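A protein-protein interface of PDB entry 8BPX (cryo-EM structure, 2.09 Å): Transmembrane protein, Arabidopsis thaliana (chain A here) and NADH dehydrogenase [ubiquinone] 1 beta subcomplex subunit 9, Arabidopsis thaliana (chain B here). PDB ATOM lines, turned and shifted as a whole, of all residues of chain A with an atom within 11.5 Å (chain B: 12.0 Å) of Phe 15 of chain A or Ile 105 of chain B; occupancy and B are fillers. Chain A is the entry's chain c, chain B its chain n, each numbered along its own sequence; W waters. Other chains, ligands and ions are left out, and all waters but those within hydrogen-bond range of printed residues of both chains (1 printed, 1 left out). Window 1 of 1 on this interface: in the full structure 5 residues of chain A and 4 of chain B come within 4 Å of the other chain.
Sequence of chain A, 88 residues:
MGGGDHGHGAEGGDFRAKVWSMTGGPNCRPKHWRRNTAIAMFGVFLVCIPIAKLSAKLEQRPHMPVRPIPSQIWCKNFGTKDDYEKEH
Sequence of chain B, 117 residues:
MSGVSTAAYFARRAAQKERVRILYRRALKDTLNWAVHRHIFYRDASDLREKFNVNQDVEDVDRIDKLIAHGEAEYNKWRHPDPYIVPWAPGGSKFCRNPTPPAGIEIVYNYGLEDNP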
ATOM      1  N   GLY A  13     -24.767 -12.351  18.008  1.00  0.00           N
ATOM      2  CA  GLY A  13     -24.252 -11.050  18.388  1.00  0.00           C
ATOM      3  C   GLY A  13     -22.762 -10.944  18.163  1.00  0.00           C
ATOM      4  O   GLY A  13     -22.295 -10.889  17.027  1.00  0.00           O
ATOM      5  N   ASP A  14     -22.005 -10.910  19.256  1.00  0.00           N
ATOM      6  CA  ASP A  14     -20.552 -10.936  19.186  1.00  0.00           C
ATOM      7  C   ASP A  14     -19.980 -12.274  19.636  1.00  0.00           C
ATOM      8  O   ASP A  14     -19.174 -12.873  18.918  1.00  0.00           O
ATOM      9  CB  ASP A  14     -19.960  -9.796  20.019  1.00  0.00           C
ATOM     10  CG  ASP A  14     -19.861  -8.498  19.240  1.00  0.00           C
ATOM     11  OD1 ASP A  14     -20.773  -7.654  19.364  1.00  0.00           O
ATOM     12  OD2 ASP A  14     -18.867  -8.321  18.505  1.00  0.00           O
ATOM     13  N   PHE A  15     -20.385 -12.766  20.806  1.00  0.00           N
ATOM     14  CA  PHE A  15     -19.897 -14.061  21.255  1.00  0.00           C
ATOM     15  C   PHE A  15     -20.569 -15.224  20.532  1.00  0.00           C
ATOM     16  O   PHE A  15     -19.969 -16.297  20.426  1.00  0.00           O
ATOM     17  CB  PHE A  15     -20.065 -14.199  22.776  1.00  0.00           C
ATOM     18  CG  PHE A  15     -21.474 -14.459  23.228  1.00  0.00           C
ATOM     19  CD1 PHE A  15     -21.989 -15.749  23.261  1.00  0.00           C
ATOM     20  CD2 PHE A  15     -22.273 -13.420  23.667  1.00  0.00           C
ATOM     21  CE1 PHE A  15     -23.277 -15.984  23.682  1.00  0.00           C
ATOM     22  CE2 PHE A  15     -23.558 -13.651  24.097  1.00  0.00           C
ATOM     23  CZ  PHE A  15     -24.062 -14.938  24.103  1.00  0.00           C
ATOM     24  N   ARG A  16     -21.791 -15.037  20.030  1.00  0.00           N
ATOM     25  CA  ARG A  16     -22.522 -16.135  19.411  1.00  0.00           C
ATOM     26  C   ARG A  16     -21.878 -16.610  18.111  1.00  0.00           C
ATOM     27  O   ARG A  16     -22.146 -17.733  17.675  1.00  0.00           O
ATOM     28  CB  ARG A  16     -23.975 -15.718  19.179  1.00  0.00           C
ATOM     29  CG  ARG A  16     -24.805 -15.667  20.468  1.00  0.00           C
ATOM     30  CD  ARG A  16     -26.264 -15.328  20.204  1.00  0.00           C
ATOM     31  NE  ARG A  16     -26.424 -14.004  19.619  1.00  0.00           N
ATOM     32  CZ  ARG A  16     -27.581 -13.372  19.480  1.00  0.00           C
ATOM     33  NH1 ARG A  16     -28.718 -13.915  19.876  1.00  0.00           N
ATOM     34  NH2 ARG A  16     -27.598 -12.166  18.925  1.00  0.00           N
ATOM     35  N   ALA A  17     -21.027 -15.791  17.493  1.00  0.00           N
ATOM     36  CA  ALA A  17     -20.267 -16.218  16.326  1.00  0.00           C
ATOM     37  C   ALA A  17     -19.233 -17.284  16.660  1.00  0.00           C
ATOM     38  O   ALA A  17     -18.706 -17.919  15.745  1.00  0.00           O
ATOM     39  CB  ALA A  17     -19.575 -15.020  15.681  1.00  0.00           C
ATOM     40  N   LYS A  18     -18.926 -17.489  17.935  1.00  0.00           N
ATOM     41  CA  LYS A  18     -18.011 -18.535  18.352  1.00  0.00           C
ATOM     42  C   LYS A  18     -18.735 -19.748  18.916  1.00  0.00           C
ATOM     43  O   LYS A  18     -18.087 -20.638  19.474  1.00  0.00           O
ATOM     44  CB  LYS A  18     -17.023 -17.986  19.380  1.00  0.00           C
ATOM     45  CG  LYS A  18     -16.430 -16.647  18.994  1.00  0.00           C
ATOM     46  CD  LYS A  18     -15.783 -15.972  20.181  1.00  0.00           C
ATOM     47  CE  LYS A  18     -14.366 -16.472  20.391  1.00  0.00           C
ATOM     48  NZ  LYS A  18     -14.307 -17.662  21.269  1.00  0.00           N
ATOM     49  N   VAL A  19     -20.054 -19.808  18.785  1.00  0.00           N
ATOM     50  CA  VAL A  19     -20.856 -20.855  19.402  1.00  0.00           C
ATOM     51  C   VAL A  19     -21.414 -21.738  18.294  1.00  0.00           C
ATOM     52  O   VAL A  19     -22.154 -21.267  17.424  1.00  0.00           O
ATOM     53  CB  VAL A  19     -21.982 -20.268  20.268  1.00  0.00           C
ATOM     54  CG1 VAL A  19     -23.025 -21.332  20.586  1.00  0.00           C
ATOM     55  CG2 VAL A  19     -21.414 -19.640  21.536  1.00  0.00           C
ATOM     56  N   TRP A  20     -21.066 -23.018  18.335  1.00  0.00           N
ATOM     57  CA  TRP A  20     -21.502 -23.992  17.345  1.00  0.00           C
ATOM     58  C   TRP A  20     -22.844 -24.580  17.762  1.00  0.00           C
ATOM     59  O   TRP A  20     -23.026 -24.954  18.922  1.00  0.00           O
ATOM     60  CB  TRP A  20     -20.446 -25.093  17.207  1.00  0.00           C
ATOM     61  CG  TRP A  20     -20.641 -26.036  16.053  1.00  0.00           C
ATOM     62  CD1 TRP A  20     -19.981 -26.012  14.862  1.00  0.00           C
ATOM     63  CD2 TRP A  20     -21.531 -27.157  15.995  1.00  0.00           C
ATOM     64  NE1 TRP A  20     -20.412 -27.036  14.062  1.00  0.00           N
ATOM     65  CE2 TRP A  20     -21.363 -27.756  14.732  1.00  0.00           C
ATOM     66  CE3 TRP A  20     -22.459 -27.709  16.885  1.00  0.00           C
ATOM     67  CZ2 TRP A  20     -22.088 -28.878  14.335  1.00  0.00           C
ATOM     68  CZ3 TRP A  20     -23.172 -28.822  16.492  1.00  0.00           C
ATOM     69  CH2 TRP A  20     -22.986 -29.394  15.227  1.00  0.00           C
ATOM     70  N   SER A  21     -23.790 -24.640  16.823  1.00  0.00           N
ATOM     71  CA  SER A  21     -25.050 -25.339  17.039  1.00  0.00           C
ATOM     72  C   SER A  21     -25.428 -26.104  15.778  1.00  0.00           C
ATOM     73  O   SER A  21     -24.963 -25.802  14.678  1.00  0.00           O
ATOM     74  CB  SER A  21     -26.195 -24.392  17.436  1.00  0.00           C
ATOM     75  OG  SER A  21     -26.350 -23.336  16.514  1.00  0.00           O
ATOM     76  N   GLY A  24     -27.666 -23.867  13.574  1.00  0.00           N
ATOM     77  CA  GLY A  24     -26.926 -22.806  12.932  1.00  0.00           C
ATOM     78  C   GLY A  24     -26.851 -21.495  13.686  1.00  0.00           C
ATOM     79  O   GLY A  24     -26.091 -20.618  13.272  1.00  0.00           O
ATOM     80  N   GLY A  25     -27.609 -21.324  14.761  1.00  0.00           N
ATOM     81  CA  GLY A  25     -27.567 -20.096  15.520  1.00  0.00           C
ATOM     82  C   GLY A  25     -28.264 -18.940  14.828  1.00  0.00           C
ATOM     83  O   GLY A  25     -28.978 -19.119  13.841  1.00  0.00           O
ATOM     84  N   PRO A  26     -28.056 -17.724  15.330  1.00  0.00           N
ATOM     85  CA  PRO A  26     -28.809 -16.570  14.823  1.00  0.00           C
ATOM     86  C   PRO A  26     -28.317 -16.071  13.471  1.00  0.00           C
ATOM     87  O   PRO A  26     -27.114 -15.937  13.234  1.00  0.00           O
ATOM     88  CB  PRO A  26     -28.590 -15.511  15.910  1.00  0.00           C
ATOM     89  CG  PRO A  26     -27.273 -15.868  16.507  1.00  0.00           C
ATOM     90  CD  PRO A  26     -27.164 -17.360  16.445  1.00  0.00           C
ATOM     91  N   ASN B  98     -35.820 -11.215  21.366  1.00  0.00           N
ATOM     92  CA  ASN B  98     -34.567 -11.023  20.592  1.00  0.00           C
ATOM     93  C   ASN B  98     -33.689  -9.895  21.183  1.00  0.00           C
ATOM     94  O   ASN B  98     -33.310  -9.040  20.464  1.00  0.00           O
ATOM     95  CB  ASN B  98     -34.864 -10.966  19.096  1.00  0.00           C
ATOM     96  CG  ASN B  98     -35.646 -12.158  18.600  1.00  0.00           C
ATOM     97  OD1 ASN B  98     -35.395 -13.280  19.013  1.00  0.00           O
ATOM     98  ND2 ASN B  98     -36.598 -11.922  17.723  1.00  0.00           N
ATOM     99  N   PRO B  99     -33.358  -9.915  22.477  1.00  0.00           N
ATOM    100  CA  PRO B  99     -32.472  -8.886  23.026  1.00  0.00           C
ATOM    101  C   PRO B  99     -31.075  -8.976  22.443  1.00  0.00           C
ATOM    102  O   PRO B  99     -30.622 -10.035  22.005  1.00  0.00           O
ATOM    103  CB  PRO B  99     -32.463  -9.197  24.524  1.00  0.00           C
ATOM    104  CG  PRO B  99     -32.696 -10.668  24.588  1.00  0.00           C
ATOM    105  CD  PRO B  99     -33.598 -11.010  23.434  1.00  0.00           C
ATOM    106  N   THR B 100     -30.399  -7.839  22.436  1.00  0.00           N
ATOM    107  CA  THR B 100     -28.988  -7.844  22.104  1.00  0.00           C
ATOM    108  C   THR B 100     -28.228  -8.638  23.162  1.00  0.00           C
ATOM    109  O   THR B 100     -28.558  -8.562  24.350  1.00  0.00           O
ATOM    110  CB  THR B 100     -28.440  -6.418  22.011  1.00  0.00           C
ATOM    111  OG1 THR B 100     -29.133  -5.708  20.977  1.00  0.00           O
ATOM    112  CG2 THR B 100     -26.964  -6.432  21.696  1.00  0.00           C
ATOM    113  N   PRO B 101     -27.233  -9.429  22.766  1.00  0.00           N
ATOM    114  CA  PRO B 101     -26.517 -10.237  23.744  1.00  0.00           C
ATOM    115  C   PRO B 101     -25.758  -9.357  24.715  1.00  0.00           C
ATOM    116  O   PRO B 101     -25.326  -8.242  24.367  1.00  0.00           O
ATOM    117  CB  PRO B 101     -25.563 -11.074  22.880  1.00  0.00           C
ATOM    118  CG  PRO B 101     -26.047 -10.950  21.495  1.00  0.00           C
ATOM    119  CD  PRO B 101     -26.773  -9.660  21.389  1.00  0.00           C
ATOM    120  N   PRO B 102     -25.575  -9.813  25.948  1.00  0.00           N
ATOM    121  CA  PRO B 102     -24.731  -9.069  26.889  1.00  0.00           C
ATOM    122  C   PRO B 102     -23.283  -9.051  26.430  1.00  0.00           C
ATOM    123  O   PRO B 102     -22.813  -9.953  25.733  1.00  0.00           O
ATOM    124  CB  PRO B 102     -24.883  -9.841  28.204  1.00  0.00           C
ATOM    125  CG  PRO B 102     -25.364 -11.197  27.817  1.00  0.00           C
ATOM    126  CD  PRO B 102     -26.073 -11.084  26.501  1.00  0.00           C
ATOM    127  N   ALA B 103     -22.581  -7.993  26.817  1.00  0.00           N
ATOM    128  CA  ALA B 103     -21.149  -7.919  26.597  1.00  0.00           C
ATOM    129  C   ALA B 103     -20.402  -8.612  27.734  1.00  0.00           C
ATOM    130  O   ALA B 103     -20.930  -8.807  28.832  1.00  0.00           O
ATOM    131  CB  ALA B 103     -20.694  -6.467  26.477  1.00  0.00           C
ATOM    132  N   GLY B 104     -19.158  -8.983  27.457  1.00  0.00           N
ATOM    133  CA  GLY B 104     -18.331  -9.648  28.442  1.00  0.00           C
ATOM    134  C   GLY B 104     -18.425 -11.155  28.466  1.00  0.00           C
ATOM    135  O   GLY B 104     -18.022 -11.769  29.459  1.00  0.00           O
ATOM    136  N   ILE B 105     -18.939 -11.773  27.410  1.00  0.00           N
ATOM    137  CA  ILE B 105     -19.103 -13.218  27.343  1.00  0.00           C
ATOM    138  C   ILE B 105     -17.947 -13.785  26.538  1.00  0.00           C
ATOM    139  O   ILE B 105     -17.688 -13.343  25.415  1.00  0.00           O
ATOM    140  CB  ILE B 105     -20.453 -13.599  26.710  1.00  0.00           C
ATOM    141  CG1 ILE B 105     -21.614 -13.101  27.572  1.00  0.00           C
ATOM    142  CG2 ILE B 105     -20.538 -15.106  26.499  1.00  0.00           C
ATOM    143  CD1 ILE B 105     -21.470 -13.388  29.048  1.00  0.00           C
ATOM    144  N   GLU B 106     -17.234 -14.717  27.155  1.00  0.00           N
ATOM    145  CA  GLU B 106     -16.103 -15.415  26.510  1.00  0.00           C
ATOM    146  C   GLU B 106     -16.442 -16.901  26.264  1.00  0.00           C
ATOM    147  O   GLU B 106     -17.041 -17.504  27.134  1.00  0.00           O
ATOM    148  CB  GLU B 106     -14.873 -15.182  27.372  1.00  0.00           C
ATOM    149  CG  GLU B 106     -14.550 -13.726  27.559  1.00  0.00           C
ATOM    150  CD  GLU B 106     -13.782 -13.388  28.818  1.00  0.00           C
ATOM    151  OE1 GLU B 106     -12.814 -14.087  29.112  1.00  0.00           O
ATOM    152  OE2 GLU B 106     -14.151 -12.400  29.488  1.00  0.00           O
ATOM    153  N   ILE B 107     -16.110 -17.453  25.124  1.00  0.00           N
ATOM    154  CA  ILE B 107     -16.318 -18.863  24.822  1.00  0.00           C
ATOM    155  C   ILE B 107     -14.956 -19.537  24.811  1.00  0.00           C
ATOM    156  O   ILE B 107     -14.033 -19.068  24.136  1.00  0.00           O
ATOM    157  CB  ILE B 107     -17.033 -19.044  23.470  1.00  0.00           C
ATOM    158  CG1 ILE B 107     -18.410 -18.368  23.475  1.00  0.00           C
ATOM    159  CG2 ILE B 107     -17.161 -20.514  23.124  1.00  0.00           C
ATOM    160  CD1 ILE B 107     -19.322 -18.783  24.598  1.00  0.00           C
ATOM    161  N   VAL B 108     -14.800 -20.615  25.539  1.00  0.00           N
ATOM    162  CA  VAL B 108     -13.471 -21.287  25.672  1.00  0.00           C
ATOM    163  C   VAL B 108     -13.453 -22.501  24.756  1.00  0.00           C
ATOM    164  O   VAL B 108     -14.438 -23.235  24.671  1.00  0.00           O
ATOM    165  CB  VAL B 108     -13.105 -21.698  27.126  1.00  0.00           C
ATOM    166  CG1 VAL B 108     -11.725 -22.281  27.308  1.00  0.00           C
ATOM    167  CG2 VAL B 108     -13.453 -20.674  28.172  1.00  0.00           C
ATOM    168  N   TYR B 109     -12.338 -22.709  24.149  1.00  0.00           N
ATOM    169  CA  TYR B 109     -12.077 -23.821  23.252  1.00  0.00           C
ATOM    170  C   TYR B 109     -11.094 -24.782  23.907  1.00  0.00           C
ATOM    171  O   TYR B 109     -10.318 -24.394  24.784  1.00  0.00           O
ATOM    172  CB  TYR B 109     -11.516 -23.319  21.920  1.00  0.00           C
ATOM    173  CG  TYR B 109     -12.536 -22.623  21.054  1.00  0.00           C
ATOM    174  CD1 TYR B 109     -13.885 -22.928  21.150  1.00  0.00           C
ATOM    175  CD2 TYR B 109     -12.151 -21.625  20.173  1.00  0.00           C
ATOM    176  CE1 TYR B 109     -14.818 -22.285  20.364  1.00  0.00           C
ATOM    177  CE2 TYR B 109     -13.070 -20.974  19.389  1.00  0.00           C
ATOM    178  CZ  TYR B 109     -14.403 -21.305  19.488  1.00  0.00           C
ATOM    179  OH  TYR B 109     -15.318 -20.652  18.702  1.00  0.00           O
HETATM  180  O   HOH W   1     -14.488 -15.695  23.716  1.00  0.00           O
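Water W1 lies within hydrogen-bond range of the backbone NH of Ile 107 of chain B (2.8 Å) and the side-chain amino group of Lys 18 of chain A (3.1 Å).
Of the printed residues of chain B, Phe 15 of chain A touches Pro 101 and Ile 105. Ile 105 of chain B touches just one residue of chain A: Phe 15 (3.5 Å). No residue of chain B comes within 4 Å of Asp 14 of chain A. Of chain B, only Pro 101 (3.2 Å) comes within 4 Å of Arg 16 of chain A. Ala 17 of chain A touches none of the printed residues of chain B. Lys 18 of chain A touches just these residues of chain B: Ile 107 (3.2 Å) and Tyr 109 (2.9 Å). Pro 101 of chain B touches three residues of chain A. No residue of chain A comes within 4 Å of Ala 103 of chain B. Glu 106 of chain B touches none of the printed residues of chain A. Of the printed residues of chain A, Ile 107 of chain B touches Lys 18 (3.2 Å) and Val 19 (3.8 Å). Printed residues of chain A within 4 Å of Tyr 109 of chain B: Lys 18 (2.9 Å). Ser 21 of chain A touches none of the printed residues of chain B. Asn 98 of chain B touches none of the printed residues of chain A. The nearest printed residue of chain B that does not touch Phe 15 of chain A is Ile 107 of chain B (4.002 Å). The nearest residue of chain A that does not touch Ile 105 of chain B is Lys 18 of chain A (6.2 Å).
Among the printed residues, pairs that only touch across the chains: Gly 13 of chain A with Pro 101 of chain B, Phe 15 of chain A with Pro 101 of chain B, Phe 15 of chain A with Ile 105 of chain B, Arg 16 of chain A with Pro 101 of chain B and Val 19 of chain A with Ile 107 of chain B.
Hydrophobic or aromatic side chains of chain A within 4 Å of the printed part of chain B: Phe 15 and Val 19.
The backbone carbonyl oxygen (O) of Lys 18 of chain A lies within hydrogen-bond range of the side-chain hydroxyl (OH) of Tyr 109 of chain B. The backbone carbonyl oxygen of Ile 107 of chain B lies within hydrogen-bond range of the side-chain amino group of Lys 18 of chain A (3.2 Å).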
